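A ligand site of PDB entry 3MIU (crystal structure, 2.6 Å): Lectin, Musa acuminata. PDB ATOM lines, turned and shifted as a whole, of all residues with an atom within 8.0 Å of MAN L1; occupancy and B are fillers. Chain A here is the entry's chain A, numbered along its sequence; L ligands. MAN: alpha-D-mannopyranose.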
ATOM      1  N   PHE A  32     -17.047 -25.915 -28.894  1.00  0.00           N
ATOM      2  CA  PHE A  32     -15.642 -25.535 -29.039  1.00  0.00           C
ATOM      3  C   PHE A  32     -15.264 -24.577 -27.910  1.00  0.00           C
ATOM      4  O   PHE A  32     -15.864 -23.515 -27.772  1.00  0.00           O
ATOM      5  CB  PHE A  32     -15.412 -24.842 -30.378  1.00  0.00           C
ATOM      6  CG  PHE A  32     -15.566 -25.741 -31.581  1.00  0.00           C
ATOM      7  CD1 PHE A  32     -14.442 -26.240 -32.226  1.00  0.00           C
ATOM      8  CD2 PHE A  32     -16.826 -26.056 -32.076  1.00  0.00           C
ATOM      9  CE1 PHE A  32     -14.569 -27.054 -33.346  1.00  0.00           C
ATOM     10  CE2 PHE A  32     -16.958 -26.878 -33.194  1.00  0.00           C
ATOM     11  CZ  PHE A  32     -15.826 -27.379 -33.828  1.00  0.00           C
ATOM     12  N   SER A  33     -14.269 -24.952 -27.105  1.00  0.00           N
ATOM     13  CA  SER A  33     -13.834 -24.081 -26.021  1.00  0.00           C
ATOM     14  C   SER A  33     -12.367 -24.198 -25.710  1.00  0.00           C
ATOM     15  O   SER A  33     -11.725 -25.216 -26.011  1.00  0.00           O
ATOM     16  CB  SER A  33     -14.640 -24.365 -24.755  1.00  0.00           C
ATOM     17  OG  SER A  33     -14.399 -25.686 -24.288  1.00  0.00           O
ATOM     18  N   GLY A  34     -11.824 -23.136 -25.105  1.00  0.00           N
ATOM     19  CA  GLY A  34     -10.478 -23.137 -24.573  1.00  0.00           C
ATOM     20  C   GLY A  34     -10.574 -22.516 -23.199  1.00  0.00           C
ATOM     21  O   GLY A  34     -11.148 -23.109 -22.282  1.00  0.00           O
ATOM     22  N   ASP A  35     -10.009 -21.315 -23.054  1.00  0.00           N
ATOM     23  CA  ASP A  35     -10.189 -20.465 -21.891  1.00  0.00           C
ATOM     24  C   ASP A  35     -11.639 -20.094 -21.761  1.00  0.00           C
ATOM     25  O   ASP A  35     -12.158 -19.934 -20.665  1.00  0.00           O
ATOM     26  CB  ASP A  35      -9.430 -19.149 -22.096  1.00  0.00           C
ATOM     27  CG  ASP A  35      -7.955 -19.270 -21.834  1.00  0.00           C
ATOM     28  OD1 ASP A  35      -7.245 -18.265 -22.054  1.00  0.00           O
ATOM     29  OD2 ASP A  35      -7.508 -20.351 -21.407  1.00  0.00           O
ATOM     30  N   VAL A  36     -12.284 -19.953 -22.917  1.00  0.00           N
ATOM     31  CA  VAL A  36     -13.621 -19.413 -23.052  1.00  0.00           C
ATOM     32  C   VAL A  36     -14.394 -20.290 -24.042  1.00  0.00           C
ATOM     33  O   VAL A  36     -13.794 -21.062 -24.784  1.00  0.00           O
ATOM     34  CB  VAL A  36     -13.510 -17.941 -23.547  1.00  0.00           C
ATOM     35  CG1 VAL A  36     -14.662 -17.543 -24.472  1.00  0.00           C
ATOM     36  CG2 VAL A  36     -13.409 -16.991 -22.351  1.00  0.00           C
ATOM     37  N   VAL A  37     -15.715 -20.195 -24.058  1.00  0.00           N
ATOM     38  CA  VAL A  37     -16.485 -20.893 -25.074  1.00  0.00           C
ATOM     39  C   VAL A  37     -16.398 -20.146 -26.415  1.00  0.00           C
ATOM     40  O   VAL A  37     -16.921 -19.038 -26.555  1.00  0.00           O
ATOM     41  CB  VAL A  37     -17.960 -21.130 -24.671  1.00  0.00           C
ATOM     42  CG1 VAL A  37     -18.630 -22.053 -25.673  1.00  0.00           C
ATOM     43  CG2 VAL A  37     -18.041 -21.755 -23.289  1.00  0.00           C
ATOM     44  N   ASP A  38     -15.706 -20.753 -27.382  1.00  0.00           N
ATOM     45  CA  ASP A  38     -15.470 -20.121 -28.673  1.00  0.00           C
ATOM     46  C   ASP A  38     -16.670 -20.205 -29.588  1.00  0.00           C
ATOM     47  O   ASP A  38     -16.967 -19.260 -30.312  1.00  0.00           O
ATOM     48  CB  ASP A  38     -14.289 -20.780 -29.377  1.00  0.00           C
ATOM     49  CG  ASP A  38     -13.001 -20.587 -28.640  1.00  0.00           C
ATOM     50  OD1 ASP A  38     -12.802 -21.271 -27.618  1.00  0.00           O
ATOM     51  OD2 ASP A  38     -12.165 -19.763 -29.094  1.00  0.00           O
ATOM     52  N   ALA A  39     -17.354 -21.347 -29.559  1.00  0.00           N
ATOM     53  CA  ALA A  39     -18.403 -21.607 -30.532  1.00  0.00           C
ATOM     54  C   ALA A  39     -19.175 -22.880 -30.267  1.00  0.00           C
ATOM     55  O   ALA A  39     -18.823 -23.683 -29.400  1.00  0.00           O
ATOM     56  CB  ALA A  39     -17.810 -21.665 -31.919  1.00  0.00           C
ATOM     57  N   GLY A  57     -16.830 -18.528 -33.170  1.00  0.00           N
ATOM     58  CA  GLY A  57     -15.567 -18.558 -33.920  1.00  0.00           C
ATOM     59  C   GLY A  57     -14.927 -19.933 -34.065  1.00  0.00           C
ATOM     60  O   GLY A  57     -15.525 -20.955 -33.710  1.00  0.00           O
ATOM     61  N   SER A  58     -13.685 -19.951 -34.561  1.00  0.00           N
ATOM     62  CA  SER A  58     -13.026 -21.214 -34.932  1.00  0.00           C
ATOM     63  C   SER A  58     -11.954 -21.705 -33.946  1.00  0.00           C
ATOM     64  O   SER A  58     -11.293 -22.732 -34.192  1.00  0.00           O
ATOM     65  CB  SER A  58     -12.462 -21.113 -36.352  1.00  0.00           C
ATOM     66  OG  SER A  58     -11.662 -19.946 -36.505  1.00  0.00           O
ATOM     67  N   GLY A  59     -11.804 -20.989 -32.840  1.00  0.00           N
ATOM     68  CA  GLY A  59     -10.880 -21.384 -31.785  1.00  0.00           C
ATOM     69  C   GLY A  59     -11.451 -22.507 -30.946  1.00  0.00           C
ATOM     70  O   GLY A  59     -12.618 -22.883 -31.087  1.00  0.00           O
ATOM     71  N   GLY A  60     -10.625 -23.050 -30.055  1.00  0.00           N
ATOM     72  CA  GLY A  60     -11.097 -24.030 -29.071  1.00  0.00           C
ATOM     73  C   GLY A  60     -10.988 -25.480 -29.479  1.00  0.00           C
ATOM     74  O   GLY A  60     -10.738 -25.803 -30.653  1.00  0.00           O
ATOM     75  N   THR A  61     -11.169 -26.351 -28.495  1.00  0.00           N
ATOM     76  CA  THR A  61     -11.257 -27.797 -28.689  1.00  0.00           C
ATOM     77  C   THR A  61     -12.729 -28.203 -28.615  1.00  0.00           C
ATOM     78  O   THR A  61     -13.442 -27.792 -27.691  1.00  0.00           O
ATOM     79  CB  THR A  61     -10.439 -28.539 -27.623  1.00  0.00           C
ATOM     80  OG1 THR A  61      -9.101 -28.031 -27.619  1.00  0.00           O
ATOM     81  CG2 THR A  61     -10.406 -30.042 -27.887  1.00  0.00           C
ATOM     82  N   TYR A  83     -13.785 -11.080 -20.700  1.00  0.00           N
ATOM     83  CA  TYR A  83     -12.582 -11.809 -21.052  1.00  0.00           C
ATOM     84  C   TYR A  83     -11.794 -10.932 -22.000  1.00  0.00           C
ATOM     85  O   TYR A  83     -12.110 -10.874 -23.196  1.00  0.00           O
ATOM     86  CB  TYR A  83     -12.927 -13.149 -21.695  1.00  0.00           C
ATOM     87  CG  TYR A  83     -11.737 -13.941 -22.198  1.00  0.00           C
ATOM     88  CD1 TYR A  83     -10.822 -14.508 -21.305  1.00  0.00           C
ATOM     89  CD2 TYR A  83     -11.514 -14.119 -23.566  1.00  0.00           C
ATOM     90  CE1 TYR A  83      -9.724 -15.238 -21.757  1.00  0.00           C
ATOM     91  CE2 TYR A  83     -10.424 -14.850 -24.039  1.00  0.00           C
ATOM     92  CZ  TYR A  83      -9.527 -15.404 -23.131  1.00  0.00           C
ATOM     93  OH  TYR A  83      -8.440 -16.124 -23.565  1.00  0.00           O
ATOM     94  N   VAL A  88     -18.352 -12.589 -22.658  1.00  0.00           N
ATOM     95  CA  VAL A  88     -18.587 -13.835 -23.391  1.00  0.00           C
ATOM     96  C   VAL A  88     -18.942 -14.981 -22.449  1.00  0.00           C
ATOM     97  O   VAL A  88     -18.720 -14.881 -21.238  1.00  0.00           O
ATOM     98  CB  VAL A  88     -17.352 -14.274 -24.222  1.00  0.00           C
ATOM     99  CG1 VAL A  88     -17.118 -13.350 -25.404  1.00  0.00           C
ATOM    100  CG2 VAL A  88     -16.115 -14.358 -23.343  1.00  0.00           C
ATOM    101  N   VAL A  89     -19.488 -16.055 -23.009  1.00  0.00           N
ATOM    102  CA  VAL A  89     -19.737 -17.263 -22.240  1.00  0.00           C
ATOM    103  C   VAL A  89     -18.380 -17.923 -21.927  1.00  0.00           C
ATOM    104  O   VAL A  89     -17.714 -18.441 -22.826  1.00  0.00           O
ATOM    105  CB  VAL A  89     -20.742 -18.211 -22.977  1.00  0.00           C
ATOM    106  CG1 VAL A  89     -20.696 -19.612 -22.408  1.00  0.00           C
ATOM    107  CG2 VAL A  89     -22.172 -17.692 -22.864  1.00  0.00           C
ATOM    108  N   GLY A  90     -17.970 -17.879 -20.669  1.00  0.00           N
ATOM    109  CA  GLY A  90     -16.685 -18.446 -20.271  1.00  0.00           C
ATOM    110  C   GLY A  90     -16.729 -19.907 -19.920  1.00  0.00           C
ATOM    111  O   GLY A  90     -15.723 -20.604 -19.993  1.00  0.00           O
ATOM    112  N   GLY A 105     -14.926 -24.848 -20.906  1.00  0.00           N
ATOM    113  CA  GLY A 105     -14.398 -23.504 -20.729  1.00  0.00           C
ATOM    114  C   GLY A 105     -13.821 -23.394 -19.342  1.00  0.00           C
ATOM    115  O   GLY A 105     -14.270 -24.075 -18.415  1.00  0.00           O
ATOM    116  N   ASN A 106     -12.810 -22.524 -19.185  1.00  0.00           N
ATOM    117  CA  ASN A 106     -12.053 -22.403 -17.936  1.00  0.00           C
ATOM    118  C   ASN A 106     -12.069 -20.999 -17.312  1.00  0.00           C
ATOM    119  O   ASN A 106     -11.289 -20.714 -16.405  1.00  0.00           O
ATOM    120  CB  ASN A 106     -10.612 -22.892 -18.149  1.00  0.00           C
ATOM    121  CG  ASN A 106     -10.543 -24.334 -18.614  1.00  0.00           C
ATOM    122  OD1 ASN A 106     -11.308 -25.193 -18.147  1.00  0.00           O
ATOM    123  ND2 ASN A 106      -9.615 -24.628 -19.534  1.00  0.00           N
ATOM    124  N   THR A 107     -12.966 -20.139 -17.793  1.00  0.00           N
ATOM    125  CA  THR A 107     -13.079 -18.787 -17.266  1.00  0.00           C
ATOM    126  C   THR A 107     -14.412 -18.584 -16.535  1.00  0.00           C
ATOM    127  O   THR A 107     -15.488 -18.573 -17.146  1.00  0.00           O
ATOM    128  CB  THR A 107     -12.903 -17.722 -18.375  1.00  0.00           C
ATOM    129  OG1 THR A 107     -11.609 -17.860 -18.970  1.00  0.00           O
ATOM    130  CG2 THR A 107     -13.046 -16.320 -17.800  1.00  0.00           C
ATOM    131  N   ASP A 130     -15.867 -13.964 -32.632  1.00  0.00           N
ATOM    132  CA  ASP A 130     -14.841 -15.002 -32.624  1.00  0.00           C
ATOM    133  C   ASP A 130     -14.967 -15.892 -31.393  1.00  0.00           C
ATOM    134  O   ASP A 130     -14.327 -16.948 -31.311  1.00  0.00           O
ATOM    135  CB  ASP A 130     -13.422 -14.408 -32.762  1.00  0.00           C
ATOM    136  CG  ASP A 130     -13.065 -13.454 -31.654  1.00  0.00           C
ATOM    137  OD1 ASP A 130     -13.907 -13.269 -30.752  1.00  0.00           O
ATOM    138  OD2 ASP A 130     -11.949 -12.880 -31.681  1.00  0.00           O
ATOM    139  N   PHE A 131     -15.776 -15.455 -30.430  1.00  0.00           N
ATOM    140  CA  PHE A 131     -16.204 -16.265 -29.302  1.00  0.00           C
ATOM    141  C   PHE A 131     -17.728 -16.249 -29.228  1.00  0.00           C
ATOM    142  O   PHE A 131     -18.379 -15.501 -29.974  1.00  0.00           O
ATOM    143  CB  PHE A 131     -15.637 -15.725 -27.988  1.00  0.00           C
ATOM    144  CG  PHE A 131     -14.136 -15.571 -27.984  1.00  0.00           C
ATOM    145  CD1 PHE A 131     -13.563 -14.356 -27.604  1.00  0.00           C
ATOM    146  CD2 PHE A 131     -13.313 -16.624 -28.368  1.00  0.00           C
ATOM    147  CE1 PHE A 131     -12.173 -14.200 -27.597  1.00  0.00           C
ATOM    148  CE2 PHE A 131     -11.915 -16.473 -28.360  1.00  0.00           C
ATOM    149  CZ  PHE A 131     -11.343 -15.255 -27.970  1.00  0.00           C
HETATM  150  C1  MAN L   1      -7.096 -21.004 -25.767  1.00  0.00           C
HETATM  151  C2  MAN L   1      -7.119 -21.853 -27.047  1.00  0.00           C
HETATM  152  C3  MAN L   1      -7.786 -21.151 -28.239  1.00  0.00           C
HETATM  153  C4  MAN L   1      -9.048 -20.397 -27.866  1.00  0.00           C
HETATM  154  C5  MAN L   1      -8.858 -19.561 -26.603  1.00  0.00           C
HETATM  155  C6  MAN L   1     -10.157 -18.876 -26.162  1.00  0.00           C
HETATM  156  O1  MAN L   1      -6.051 -20.040 -25.778  1.00  0.00           O
HETATM  157  O2  MAN L   1      -7.756 -23.083 -26.785  1.00  0.00           O
HETATM  158  O3  MAN L   1      -8.123 -22.092 -29.245  1.00  0.00           O
HETATM  159  O4  MAN L   1      -9.416 -19.581 -28.965  1.00  0.00           O
HETATM  160  O5  MAN L   1      -8.358 -20.378 -25.547  1.00  0.00           O
HETATM  161  O6  MAN L   1     -11.093 -19.826 -25.682  1.00  0.00           O
HETATM  162  C1  MAN L   2     -11.305 -26.661 -22.474  1.00  0.00           C
HETATM  163  C2  MAN L   2     -10.599 -27.959 -22.885  1.00  0.00           C
HETATM  164  C3  MAN L   2     -11.399 -29.209 -22.534  1.00  0.00           C
HETATM  165  C4  MAN L   2     -11.874 -29.119 -21.086  1.00  0.00           C
HETATM  166  C5  MAN L   2     -12.828 -27.926 -21.006  1.00  0.00           C
HETATM  167  C6  MAN L   2     -13.469 -27.809 -19.627  1.00  0.00           C
HETATM  168  O1  MAN L   2     -12.037 -26.170 -23.573  1.00  0.00           O
HETATM  169  O2  MAN L   2      -9.330 -28.018 -22.280  1.00  0.00           O
HETATM  170  O3  MAN L   2     -10.629 -30.366 -22.739  1.00  0.00           O
HETATM  171  O4  MAN L   2     -12.485 -30.329 -20.671  1.00  0.00           O
HETATM  172  O5  MAN L   2     -12.156 -26.715 -21.323  1.00  0.00           O
HETATM  173  O6  MAN L   2     -12.560 -27.275 -18.694  1.00  0.00           O
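N of Gly 34 lies within hydrogen-bond range of OD1 of Asp 38.
O of Phe 32 is in hydrogen-bond range of N of Asp 38.
The backbone NH (N) of Gly 57 is in hydrogen-bond range of the backbone carbonyl oxygen (O) of Asp 38 (3.0 Å).
The side-chain hydroxyl of Tyr 83 sits at hydrogen-bond distance from the side-chain carboxylate of Asp 35, at 2.9 Å.
O of Asp 35 is in hydrogen-bond range of OG1 of Thr 107 (2.7 Å).
The backbone carbonyl oxygen (O) of Asp 35 sits at hydrogen-bond distance from the backbone NH (N) of Asn 106.
O of Gly 34 sits at hydrogen-bond distance from ND2 of Asn 106, at 3.5 Å.
Gly 59 touches MAN L1.
Phe 131 touches MAN L1 (CE2 to C6, 3.7 Å).
Hydrophobic or aromatic side chains that line MAN L1: Val 36 and Phe 131.
An oxygen (O4) of MAN L1 is in hydrogen-bond range of the side-chain carboxylate (OD2) of Asp 38 (2.8 Å).
N of Gly 60 lies within hydrogen-bond range of O3 of MAN L1 (2.8 Å).
The backbone NH of Val 36 sits at hydrogen-bond distance from an oxygen (O6) of MAN L1, 3.0 Å away.
The backbone carbonyl oxygen (O) of Val 36 is in hydrogen-bond range of an oxygen (O6) of MAN L1, 3.1 Å away.
An oxygen (O5) of MAN L1 sits at hydrogen-bond distance from the backbone NH (N) of Asp 35.
O6 of MAN L1 lies within hydrogen-bond range of N of Gly 34 (3.4 Å).
The backbone NH (N) of Gly 34 sits at hydrogen-bond distance from an oxygen (O1) of MAN L2 (3.4 Å).
An oxygen (O1) of MAN L2 sits at hydrogen-bond distance from the backbone carbonyl oxygen of Gly 34.
O1 of MAN L2 lies within hydrogen-bond range of O of Ser 33.
An oxygen (O1) of MAN L2 lies within hydrogen-bond range of the side-chain hydroxyl of Ser 33 (2.5 Å).
N of Gly 105 is in hydrogen-bond range of O5 of MAN L2.
OD1 of Asn 106 is in hydrogen-bond range of O6 of MAN L2.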
